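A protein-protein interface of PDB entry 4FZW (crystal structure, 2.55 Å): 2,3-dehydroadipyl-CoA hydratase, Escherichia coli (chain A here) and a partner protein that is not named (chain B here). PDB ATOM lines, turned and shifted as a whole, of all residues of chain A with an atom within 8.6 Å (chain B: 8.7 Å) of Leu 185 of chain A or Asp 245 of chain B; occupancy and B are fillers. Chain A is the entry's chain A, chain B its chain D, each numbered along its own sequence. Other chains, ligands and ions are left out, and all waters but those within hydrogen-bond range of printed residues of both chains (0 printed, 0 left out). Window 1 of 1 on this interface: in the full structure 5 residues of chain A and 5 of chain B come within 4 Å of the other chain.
OD1 of Asp 245 of chain B is in hydrogen-bond range of OH of Tyr 189 of chain A, at 2.9 Å. NH1 of Arg 248 of chain B lies within hydrogen-bond range of OH of Tyr 189 of chain A (2.5 Å). OE2 of Glu 188 of chain A is in salt-bridge range of NH2 of Arg 252 of chain B, at 3.0 Å.
The backbone carbonyl oxygen (O) of Pro 182 of chain A is in hydrogen-bond range of the side-chain hydroxyl (OG1) of Thr 186 of chain A (3.5 Å). NH2 of Arg 244 of chain B lies within salt-bridge range of OD1 of Asp 245 of chain B (2.9 Å).
Among the printed residues, pairs that only touch across the chains: Pro 182 of chain A with Asp 245 of chain B, Pro 182 of chain A with Tyr 246 of chain B, Asp 184 of chain A with Leu 249 of chain B, Leu 185 of chain A with Asp 245 of chain B, Leu 185 of chain A with Leu 249 of chain B and Glu 188 of chain A with Arg 248 of chain B.
Printed residues of chain B within 4 Å of Pro 182 of chain A: Asp 245 and Tyr 246. Of the printed residues of chain B, Asp 184 of chain A touches Leu 249 (3.9 Å). Leu 185 of chain A touches just these residues of chain B: Asp 245 (3.5 Å) and Leu 249 (3.7 Å).
Of the 17 printed residues of chain B, 5 touch a printed residue of chain A. Of the 20 printed residues of chain A, 5 touch a printed residue of chain B. Among the printed residues, 9 pairs touch across the chains. Among the printed residues, Asp or Glu carboxylates within 4 Å of a Lys or Arg side-chain nitrogen of the other chain: Glu 188 of chain A with Arg 252 of chain B.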
ATOM      1  N   ALA A 101     -26.721  15.089  12.193  1.00  0.00           N
ATOM      2  CA  ALA A 101     -25.421  15.082  12.913  1.00  0.00           C
ATOM      3  C   ALA A 101     -25.669  14.861  14.393  1.00  0.00           C
ATOM      4  O   ALA A 101     -25.915  15.833  15.123  1.00  0.00           O
ATOM      5  CB  ALA A 101     -24.681  16.390  12.718  1.00  0.00           C
ATOM      6  N   VAL A 102     -25.605  13.596  14.827  1.00  0.00           N
ATOM      7  CA  VAL A 102     -26.066  13.201  16.166  1.00  0.00           C
ATOM      8  C   VAL A 102     -24.961  13.135  17.218  1.00  0.00           C
ATOM      9  O   VAL A 102     -24.021  12.363  17.102  1.00  0.00           O
ATOM     10  CB  VAL A 102     -26.812  11.828  16.140  1.00  0.00           C
ATOM     11  CG1 VAL A 102     -27.108  11.316  17.557  1.00  0.00           C
ATOM     12  CG2 VAL A 102     -28.115  11.904  15.303  1.00  0.00           C
ATOM     13  N   ASN A 103     -25.082  13.952  18.251  1.00  0.00           N
ATOM     14  CA  ASN A 103     -24.244  13.794  19.434  1.00  0.00           C
ATOM     15  C   ASN A 103     -25.125  13.378  20.605  1.00  0.00           C
ATOM     16  O   ASN A 103     -26.330  13.596  20.586  1.00  0.00           O
ATOM     17  CB  ASN A 103     -23.458  15.082  19.754  1.00  0.00           C
ATOM     18  CG  ASN A 103     -22.155  15.203  18.951  1.00  0.00           C
ATOM     19  OD1 ASN A 103     -21.429  14.218  18.763  1.00  0.00           O
ATOM     20  ND2 ASN A 103     -21.859  16.413  18.478  1.00  0.00           N
ATOM     21  N   VAL A 121     -24.517  10.920  10.537  1.00  0.00           N
ATOM     22  CA  VAL A 121     -23.173  10.930  11.131  1.00  0.00           C
ATOM     23  C   VAL A 121     -23.336  11.085  12.633  1.00  0.00           C
ATOM     24  O   VAL A 121     -24.005  12.014  13.105  1.00  0.00           O
ATOM     25  CB  VAL A 121     -22.277  12.083  10.610  1.00  0.00           C
ATOM     26  CG1 VAL A 121     -22.171  12.080   9.085  1.00  0.00           C
ATOM     27  CG2 VAL A 121     -22.785  13.421  11.105  1.00  0.00           C
ATOM     28  N   ALA A 122     -22.751  10.156  13.381  1.00  0.00           N
ATOM     29  CA  ALA A 122     -22.864  10.171  14.832  1.00  0.00           C
ATOM     30  C   ALA A 122     -21.525  10.498  15.539  1.00  0.00           C
ATOM     31  O   ALA A 122     -20.439  10.381  14.965  1.00  0.00           O
ATOM     32  CB  ALA A 122     -23.440   8.840  15.333  1.00  0.00           C
ATOM     33  N   GLY A 123     -21.618  10.924  16.791  1.00  0.00           N
ATOM     34  CA  GLY A 123     -20.444  11.107  17.603  1.00  0.00           C
ATOM     35  C   GLY A 123     -20.134   9.854  18.391  1.00  0.00           C
ATOM     36  O   GLY A 123     -21.043   9.034  18.621  1.00  0.00           O
ATOM     37  N   GLU A 124     -18.868   9.725  18.819  1.00  0.00           N
ATOM     38  CA  GLU A 124     -18.422   8.542  19.545  1.00  0.00           C
ATOM     39  C   GLU A 124     -19.282   8.222  20.764  1.00  0.00           C
ATOM     40  O   GLU A 124     -19.326   7.067  21.187  1.00  0.00           O
ATOM     41  CB  GLU A 124     -16.959   8.660  19.997  1.00  0.00           C
ATOM     42  CG  GLU A 124     -15.938   8.729  18.900  1.00  0.00           C
ATOM     43  CD  GLU A 124     -15.978   7.545  17.961  1.00  0.00           C
ATOM     44  OE1 GLU A 124     -16.230   6.403  18.412  1.00  0.00           O
ATOM     45  OE2 GLU A 124     -15.742   7.768  16.753  1.00  0.00           O
ATOM     46  N   VAL A 180     -18.793   7.570  12.419  1.00  0.00           N
ATOM     47  CA  VAL A 180     -18.586   7.788  13.849  1.00  0.00           C
ATOM     48  C   VAL A 180     -17.322   8.619  14.104  1.00  0.00           C
ATOM     49  O   VAL A 180     -16.223   8.176  13.847  1.00  0.00           O
ATOM     50  CB  VAL A 180     -18.571   6.471  14.665  1.00  0.00           C
ATOM     51  CG1 VAL A 180     -18.421   6.774  16.143  1.00  0.00           C
ATOM     52  CG2 VAL A 180     -19.878   5.702  14.478  1.00  0.00           C
ATOM     53  N   PHE A 181     -17.513   9.841  14.587  1.00  0.00           N
ATOM     54  CA  PHE A 181     -16.431  10.792  14.812  1.00  0.00           C
ATOM     55  C   PHE A 181     -16.334  11.167  16.283  1.00  0.00           C
ATOM     56  O   PHE A 181     -17.310  11.044  17.016  1.00  0.00           O
ATOM     57  CB  PHE A 181     -16.650  12.074  14.014  1.00  0.00           C
ATOM     58  CG  PHE A 181     -16.652  11.879  12.522  1.00  0.00           C
ATOM     59  CD1 PHE A 181     -15.544  11.369  11.863  1.00  0.00           C
ATOM     60  CD2 PHE A 181     -17.771  12.225  11.773  1.00  0.00           C
ATOM     61  CE1 PHE A 181     -15.550  11.196  10.487  1.00  0.00           C
ATOM     62  CE2 PHE A 181     -17.797  12.051  10.380  1.00  0.00           C
ATOM     63  CZ  PHE A 181     -16.677  11.535   9.742  1.00  0.00           C
ATOM     64  N   PRO A 182     -15.138  11.606  16.725  1.00  0.00           N
ATOM     65  CA  PRO A 182     -15.017  12.171  18.077  1.00  0.00           C
ATOM     66  C   PRO A 182     -16.079  13.256  18.269  1.00  0.00           C
ATOM     67  O   PRO A 182     -16.277  14.097  17.393  1.00  0.00           O
ATOM     68  CB  PRO A 182     -13.596  12.769  18.092  1.00  0.00           C
ATOM     69  CG  PRO A 182     -12.845  12.012  17.059  1.00  0.00           C
ATOM     70  CD  PRO A 182     -13.843  11.543  16.018  1.00  0.00           C
ATOM     71  N   SER A 183     -16.745  13.228  19.418  1.00  0.00           N
ATOM     72  CA  SER A 183     -17.831  14.156  19.745  1.00  0.00           C
ATOM     73  C   SER A 183     -17.618  15.615  19.334  1.00  0.00           C
ATOM     74  O   SER A 183     -18.556  16.299  18.955  1.00  0.00           O
ATOM     75  CB  SER A 183     -18.105  14.134  21.248  1.00  0.00           C
ATOM     76  OG  SER A 183     -18.253  12.804  21.686  1.00  0.00           O
ATOM     77  N   ASP A 184     -16.400  16.110  19.458  1.00  0.00           N
ATOM     78  CA  ASP A 184     -16.149  17.522  19.241  1.00  0.00           C
ATOM     79  C   ASP A 184     -16.010  17.793  17.762  1.00  0.00           C
ATOM     80  O   ASP A 184     -15.875  18.940  17.363  1.00  0.00           O
ATOM     81  CB  ASP A 184     -14.874  17.969  19.984  1.00  0.00           C
ATOM     82  CG  ASP A 184     -14.973  17.782  21.496  1.00  0.00           C
ATOM     83  OD1 ASP A 184     -16.115  17.677  22.014  1.00  0.00           O
ATOM     84  OD2 ASP A 184     -13.913  17.756  22.165  1.00  0.00           O
ATOM     85  N   LEU A 185     -16.040  16.743  16.945  1.00  0.00           N
ATOM     86  CA  LEU A 185     -15.875  16.905  15.492  1.00  0.00           C
ATOM     87  C   LEU A 185     -17.122  16.528  14.645  1.00  0.00           C
ATOM     88  O   LEU A 185     -17.202  16.855  13.463  1.00  0.00           O
ATOM     89  CB  LEU A 185     -14.626  16.147  15.014  1.00  0.00           C
ATOM     90  CG  LEU A 185     -13.306  16.777  15.451  1.00  0.00           C
ATOM     91  CD1 LEU A 185     -12.169  15.765  15.350  1.00  0.00           C
ATOM     92  CD2 LEU A 185     -12.990  18.052  14.667  1.00  0.00           C
ATOM     93  N   THR A 186     -18.079  15.839  15.260  1.00  0.00           N
ATOM     94  CA  THR A 186     -19.254  15.334  14.565  1.00  0.00           C
ATOM     95  C   THR A 186     -19.933  16.420  13.707  1.00  0.00           C
ATOM     96  O   THR A 186     -20.117  16.263  12.501  1.00  0.00           O
ATOM     97  CB  THR A 186     -20.310  14.780  15.572  1.00  0.00           C
ATOM     98  OG1 THR A 186     -19.662  14.071  16.640  1.00  0.00           O
ATOM     99  CG2 THR A 186     -21.315  13.855  14.855  1.00  0.00           C
ATOM    100  N   LEU A 187     -20.305  17.516  14.355  1.00  0.00           N
ATOM    101  CA  LEU A 187     -20.986  18.615  13.696  1.00  0.00           C
ATOM    102  C   LEU A 187     -20.175  19.208  12.553  1.00  0.00           C
ATOM    103  O   LEU A 187     -20.694  19.410  11.454  1.00  0.00           O
ATOM    104  CB  LEU A 187     -21.358  19.695  14.710  1.00  0.00           C
ATOM    105  CG  LEU A 187     -22.010  20.921  14.078  1.00  0.00           C
ATOM    106  CD1 LEU A 187     -23.113  20.485  13.120  1.00  0.00           C
ATOM    107  CD2 LEU A 187     -22.548  21.856  15.165  1.00  0.00           C
ATOM    108  N   GLU A 188     -18.903  19.480  12.813  1.00  0.00           N
ATOM    109  CA  GLU A 188     -17.996  20.003  11.794  1.00  0.00           C
ATOM    110  C   GLU A 188     -17.794  19.034  10.619  1.00  0.00           C
ATOM    111  O   GLU A 188     -17.692  19.442   9.462  1.00  0.00           O
ATOM    112  CB  GLU A 188     -16.649  20.296  12.429  1.00  0.00           C
ATOM    113  CG  GLU A 188     -15.599  20.787  11.448  1.00  0.00           C
ATOM    114  CD  GLU A 188     -14.228  20.970  12.087  1.00  0.00           C
ATOM    115  OE1 GLU A 188     -14.139  20.982  13.333  1.00  0.00           O
ATOM    116  OE2 GLU A 188     -13.243  21.109  11.331  1.00  0.00           O
ATOM    117  N   TYR A 189     -17.725  17.747  10.918  1.00  0.00           N
ATOM    118  CA  TYR A 189     -17.515  16.751   9.885  1.00  0.00           C
ATOM    119  C   TYR A 189     -18.819  16.522   9.107  1.00  0.00           C
ATOM    120  O   TYR A 189     -18.797  16.302   7.896  1.00  0.00           O
ATOM    121  CB  TYR A 189     -16.961  15.446  10.497  1.00  0.00           C
ATOM    122  CG  TYR A 189     -15.494  15.535  10.793  1.00  0.00           C
ATOM    123  CD1 TYR A 189     -14.788  16.698  10.497  1.00  0.00           C
ATOM    124  CD2 TYR A 189     -14.799  14.470  11.349  1.00  0.00           C
ATOM    125  CE1 TYR A 189     -13.446  16.809  10.740  1.00  0.00           C
ATOM    126  CE2 TYR A 189     -13.407  14.570  11.617  1.00  0.00           C
ATOM    127  CZ  TYR A 189     -12.749  15.743  11.301  1.00  0.00           C
ATOM    128  OH  TYR A 189     -11.405  15.864  11.551  1.00  0.00           O
ATOM    129  N   ALA A 190     -19.941  16.590   9.816  1.00  0.00           N
ATOM    130  CA  ALA A 190     -21.262  16.535   9.196  1.00  0.00           C
ATOM    131  C   ALA A 190     -21.470  17.639   8.151  1.00  0.00           C
ATOM    132  O   ALA A 190     -22.069  17.406   7.097  1.00  0.00           O
ATOM    133  CB  ALA A 190     -22.353  16.596  10.271  1.00  0.00           C
ATOM    134  N   LEU A 191     -20.975  18.833   8.471  1.00  0.00           N
ATOM    135  CA  LEU A 191     -21.085  20.007   7.616  1.00  0.00           C
ATOM    136  C   LEU A 191     -20.199  19.916   6.394  1.00  0.00           C
ATOM    137  O   LEU A 191     -20.569  20.391   5.316  1.00  0.00           O
ATOM    138  CB  LEU A 191     -20.731  21.262   8.406  1.00  0.00           C
ATOM    139  CG  LEU A 191     -21.809  21.710   9.388  1.00  0.00           C
ATOM    140  CD1 LEU A 191     -21.289  22.844  10.250  1.00  0.00           C
ATOM    141  CD2 LEU A 191     -23.105  22.097   8.619  1.00  0.00           C
ATOM    142  N   GLN A 192     -19.017  19.327   6.573  1.00  0.00           N
ATOM    143  CA  GLN A 192     -18.129  19.056   5.451  1.00  0.00           C
ATOM    144  C   GLN A 192     -18.773  18.023   4.527  1.00  0.00           C
ATOM    145  O   GLN A 192     -18.797  18.207   3.311  1.00  0.00           O
ATOM    146  CB  GLN A 192     -16.773  18.565   5.933  1.00  0.00           C
ATOM    147  N   PHE B 219      -5.802  18.983  28.336  1.00  0.00           N
ATOM    148  CA  PHE B 219      -6.598  18.604  27.193  1.00  0.00           C
ATOM    149  C   PHE B 219      -5.768  17.740  26.270  1.00  0.00           C
ATOM    150  O   PHE B 219      -6.205  16.658  25.855  1.00  0.00           O
ATOM    151  CB  PHE B 219      -7.126  19.840  26.447  1.00  0.00           C
ATOM    152  CG  PHE B 219      -8.015  19.509  25.287  1.00  0.00           C
ATOM    153  CD1 PHE B 219      -7.552  19.628  23.987  1.00  0.00           C
ATOM    154  CD2 PHE B 219      -9.314  19.055  25.499  1.00  0.00           C
ATOM    155  CE1 PHE B 219      -8.376  19.324  22.916  1.00  0.00           C
ATOM    156  CE2 PHE B 219     -10.143  18.735  24.432  1.00  0.00           C
ATOM    157  CZ  PHE B 219      -9.670  18.866  23.141  1.00  0.00           C
ATOM    158  N   LEU B 223      -6.325  13.617  25.243  1.00  0.00           N
ATOM    159  CA  LEU B 223      -6.380  13.053  23.896  1.00  0.00           C
ATOM    160  C   LEU B 223      -5.315  11.988  23.682  1.00  0.00           C
ATOM    161  O   LEU B 223      -5.544  10.988  22.981  1.00  0.00           O
ATOM    162  CB  LEU B 223      -6.177  14.146  22.845  1.00  0.00           C
ATOM    163  CG  LEU B 223      -7.161  15.305  22.842  1.00  0.00           C
ATOM    164  CD1 LEU B 223      -6.704  16.386  21.880  1.00  0.00           C
ATOM    165  CD2 LEU B 223      -8.540  14.755  22.485  1.00  0.00           C
ATOM    166  N   THR B 238      -7.202   3.279  10.474  1.00  0.00           N
ATOM    167  CA  THR B 238      -8.132   3.921  11.376  1.00  0.00           C
ATOM    168  C   THR B 238      -7.394   4.871  12.324  1.00  0.00           C
ATOM    169  O   THR B 238      -7.839   5.996  12.539  1.00  0.00           O
ATOM    170  CB  THR B 238      -8.945   2.884  12.175  1.00  0.00           C
ATOM    171  OG1 THR B 238      -9.822   2.181  11.286  1.00  0.00           O
ATOM    172  CG2 THR B 238      -9.802   3.564  13.237  1.00  0.00           C
ATOM    173  N   GLN B 239      -6.256   4.443  12.861  1.00  0.00           N
ATOM    174  CA  GLN B 239      -5.580   5.241  13.864  1.00  0.00           C
ATOM    175  C   GLN B 239      -4.964   6.528  13.318  1.00  0.00           C
ATOM    176  O   GLN B 239      -4.741   7.474  14.080  1.00  0.00           O
ATOM    177  CB  GLN B 239      -4.521   4.409  14.626  1.00  0.00           C
ATOM    178  CG  GLN B 239      -3.981   5.090  15.884  1.00  0.00           C
ATOM    179  CD  GLN B 239      -5.001   5.164  17.011  1.00  0.00           C
ATOM    180  OE1 GLN B 239      -5.975   4.436  17.025  1.00  0.00           O
ATOM    181  NE2 GLN B 239      -4.764   6.045  17.971  1.00  0.00           N
ATOM    182  N   LEU B 240      -4.664   6.570  12.023  1.00  0.00           N
ATOM    183  CA  LEU B 240      -4.104   7.792  11.450  1.00  0.00           C
ATOM    184  C   LEU B 240      -5.193   8.861  11.291  1.00  0.00           C
ATOM    185  O   LEU B 240      -4.924  10.062  11.473  1.00  0.00           O
ATOM    186  CB  LEU B 240      -3.439   7.516  10.103  1.00  0.00           C
ATOM    187  CG  LEU B 240      -2.206   6.632  10.117  1.00  0.00           C
ATOM    188  CD1 LEU B 240      -1.980   6.090   8.734  1.00  0.00           C
ATOM    189  CD2 LEU B 240      -0.976   7.401  10.633  1.00  0.00           C
ATOM    190  N   ASP B 241      -6.409   8.415  10.962  1.00  0.00           N
ATOM    191  CA  ASP B 241      -7.564   9.294  10.934  1.00  0.00           C
ATOM    192  C   ASP B 241      -7.839   9.835  12.318  1.00  0.00           C
ATOM    193  O   ASP B 241      -8.214  10.991  12.461  1.00  0.00           O
ATOM    194  CB  ASP B 241      -8.823   8.576  10.434  1.00  0.00           C
ATOM    195  CG  ASP B 241      -8.722   8.147   8.985  1.00  0.00           C
ATOM    196  OD1 ASP B 241      -7.935   8.751   8.210  1.00  0.00           O
ATOM    197  OD2 ASP B 241      -9.445   7.197   8.614  1.00  0.00           O
ATOM    198  N   LEU B 242      -7.671   9.011  13.346  1.00  0.00           N
ATOM    199  CA  LEU B 242      -7.985   9.481  14.694  1.00  0.00           C
ATOM    200  C   LEU B 242      -6.933  10.464  15.180  1.00  0.00           C
ATOM    201  O   LEU B 242      -7.242  11.337  15.972  1.00  0.00           O
ATOM    202  CB  LEU B 242      -8.121   8.331  15.686  1.00  0.00           C
ATOM    203  CG  LEU B 242      -8.517   8.749  17.108  1.00  0.00           C
ATOM    204  CD1 LEU B 242     -10.048   8.896  17.205  1.00  0.00           C
ATOM    205  CD2 LEU B 242      -8.019   7.770  18.150  1.00  0.00           C
ATOM    206  N   GLU B 243      -5.694  10.317  14.702  1.00  0.00           N
ATOM    207  CA  GLU B 243      -4.589  11.214  15.094  1.00  0.00           C
ATOM    208  C   GLU B 243      -4.740  12.581  14.409  1.00  0.00           C
ATOM    209  O   GLU B 243      -4.594  13.645  15.038  1.00  0.00           O
ATOM    210  CB  GLU B 243      -3.202  10.608  14.781  1.00  0.00           C
ATOM    211  CG  GLU B 243      -2.813   9.375  15.553  1.00  0.00           C
ATOM    212  CD  GLU B 243      -1.326   8.981  15.371  1.00  0.00           C
ATOM    213  OE1 GLU B 243      -0.783   8.279  16.261  1.00  0.00           O
ATOM    214  OE2 GLU B 243      -0.705   9.374  14.358  1.00  0.00           O
ATOM    215  N   ARG B 244      -5.012  12.542  13.106  1.00  0.00           N
ATOM    216  CA  ARG B 244      -5.402  13.754  12.415  1.00  0.00           C
ATOM    217  C   ARG B 244      -6.509  14.436  13.207  1.00  0.00           C
ATOM    218  O   ARG B 244      -6.433  15.628  13.462  1.00  0.00           O
ATOM    219  CB  ARG B 244      -5.892  13.445  11.014  1.00  0.00           C
ATOM    220  CG  ARG B 244      -6.473  14.658  10.303  1.00  0.00           C
ATOM    221  CD  ARG B 244      -7.503  14.249   9.277  1.00  0.00           C
ATOM    222  NE  ARG B 244      -8.571  13.451   9.865  1.00  0.00           N
ATOM    223  CZ  ARG B 244      -9.392  12.675   9.160  1.00  0.00           C
ATOM    224  NH1 ARG B 244      -9.265  12.601   7.840  1.00  0.00           N
ATOM    225  NH2 ARG B 244     -10.335  11.962   9.777  1.00  0.00           N
ATOM    226  N   ASP B 245      -7.522  13.673  13.611  1.00  0.00           N
ATOM    227  CA  ASP B 245      -8.673  14.220  14.333  1.00  0.00           C
ATOM    228  C   ASP B 245      -8.250  14.881  15.632  1.00  0.00           C
ATOM    229  O   ASP B 245      -8.714  15.978  15.963  1.00  0.00           O
ATOM    230  CB  ASP B 245      -9.709  13.129  14.631  1.00  0.00           C
ATOM    231  CG  ASP B 245     -10.444  12.664  13.392  1.00  0.00           C
ATOM    232  OD1 ASP B 245     -10.331  13.339  12.351  1.00  0.00           O
ATOM    233  OD2 ASP B 245     -11.146  11.629  13.459  1.00  0.00           O
ATOM    234  N   TYR B 246      -7.374  14.210  16.376  1.00  0.00           N
ATOM    235  CA  TYR B 246      -6.968  14.715  17.682  1.00  0.00           C
ATOM    236  C   TYR B 246      -5.969  15.870  17.564  1.00  0.00           C
ATOM    237  O   TYR B 246      -5.974  16.800  18.363  1.00  0.00           O
ATOM    238  CB  TYR B 246      -6.425  13.587  18.558  1.00  0.00           C
ATOM    239  CG  TYR B 246      -7.508  12.709  19.169  1.00  0.00           C
ATOM    240  CD1 TYR B 246      -8.859  12.933  18.905  1.00  0.00           C
ATOM    241  CD2 TYR B 246      -7.174  11.670  20.021  1.00  0.00           C
ATOM    242  CE1 TYR B 246      -9.836  12.124  19.472  1.00  0.00           C
ATOM    243  CE2 TYR B 246      -8.134  10.868  20.591  1.00  0.00           C
ATOM    244  CZ  TYR B 246      -9.454  11.089  20.324  1.00  0.00           C
ATOM    245  OH  TYR B 246     -10.390  10.259  20.917  1.00  0.00           O
ATOM    246  N   GLN B 247      -5.127  15.825  16.541  1.00  0.00           N
ATOM    247  CA  GLN B 247      -4.233  16.939  16.290  1.00  0.00           C
ATOM    248  C   GLN B 247      -5.022  18.177  15.925  1.00  0.00           C
ATOM    249  O   GLN B 247      -4.793  19.252  16.488  1.00  0.00           O
ATOM    250  CB  GLN B 247      -3.244  16.625  15.171  1.00  0.00           C
ATOM    251  CG  GLN B 247      -1.920  17.335  15.375  1.00  0.00           C
ATOM    252  CD  GLN B 247      -1.145  16.777  16.573  1.00  0.00           C
ATOM    253  OE1 GLN B 247      -1.671  16.651  17.679  1.00  0.00           O
ATOM    254  NE2 GLN B 247       0.110  16.437  16.341  1.00  0.00           N
ATOM    255  N   ARG B 248      -5.941  18.015  14.972  1.00  0.00           N
ATOM    256  CA  ARG B 248      -6.834  19.097  14.561  1.00  0.00           C
ATOM    257  C   ARG B 248      -7.440  19.782  15.789  1.00  0.00           C
ATOM    258  O   ARG B 248      -7.416  21.010  15.888  1.00  0.00           O
ATOM    259  CB  ARG B 248      -7.923  18.566  13.619  1.00  0.00           C
ATOM    260  CG  ARG B 248      -9.140  19.475  13.413  1.00  0.00           C
ATOM    261  CD  ARG B 248      -9.953  19.040  12.186  1.00  0.00           C
ATOM    262  NE  ARG B 248      -9.209  19.201  10.943  1.00  0.00           N
ATOM    263  CZ  ARG B 248      -9.233  18.329   9.936  1.00  0.00           C
ATOM    264  NH1 ARG B 248      -9.972  17.228  10.024  1.00  0.00           N
ATOM    265  NH2 ARG B 248      -8.521  18.552   8.834  1.00  0.00           N
ATOM    266  N   LEU B 249      -7.944  18.985  16.732  1.00  0.00           N
ATOM    267  CA  LEU B 249      -8.507  19.511  17.976  1.00  0.00           C
ATOM    268  C   LEU B 249      -7.460  20.147  18.879  1.00  0.00           C
ATOM    269  O   LEU B 249      -7.652  21.272  19.361  1.00  0.00           O
ATOM    270  CB  LEU B 249      -9.247  18.421  18.754  1.00  0.00           C
ATOM    271  CG  LEU B 249     -10.546  17.948  18.098  1.00  0.00           C
ATOM    272  CD1 LEU B 249     -11.302  16.934  18.976  1.00  0.00           C
ATOM    273  CD2 LEU B 249     -11.429  19.163  17.803  1.00  0.00           C
ATOM    274  N   ALA B 250      -6.360  19.429  19.115  1.00  0.00           N
ATOM    275  CA  ALA B 250      -5.310  19.910  20.022  1.00  0.00           C
ATOM    276  C   ALA B 250      -4.782  21.266  19.576  1.00  0.00           C
ATOM    277  O   ALA B 250      -4.617  22.166  20.387  1.00  0.00           O
ATOM    278  CB  ALA B 250      -4.182  18.912  20.129  1.00  0.00           C
ATOM    279  N   GLY B 251      -4.534  21.412  18.280  1.00  0.00           N
ATOM    280  CA  GLY B 251      -3.987  22.649  17.731  1.00  0.00           C
ATOM    281  C   GLY B 251      -4.896  23.880  17.769  1.00  0.00           C
ATOM    282  O   GLY B 251      -4.543  24.921  17.222  1.00  0.00           O
ATOM    283  N   ARG B 252      -6.062  23.765  18.395  1.00  0.00           N
ATOM    284  CA  ARG B 252      -6.961  24.888  18.531  1.00  0.00           C
ATOM    285  C   ARG B 252      -7.028  25.255  20.002  1.00  0.00           C
ATOM    286  O   ARG B 252      -7.580  26.286  20.373  1.00  0.00           O
ATOM    287  CB  ARG B 252      -8.378  24.552  18.012  1.00  0.00           C
ATOM    288  CG  ARG B 252      -8.534  24.453  16.470  1.00  0.00           C
ATOM    289  CD  ARG B 252      -9.818  23.716  16.118  1.00  0.00           C
ATOM    290  NE  ARG B 252     -10.028  23.519  14.684  1.00  0.00           N
ATOM    291  CZ  ARG B 252     -11.018  22.786  14.175  1.00  0.00           C
ATOM    292  NH1 ARG B 252     -11.871  22.173  14.986  1.00  0.00           N
ATOM    293  NH2 ARG B 252     -11.156  22.655  12.858  1.00  0.00           N
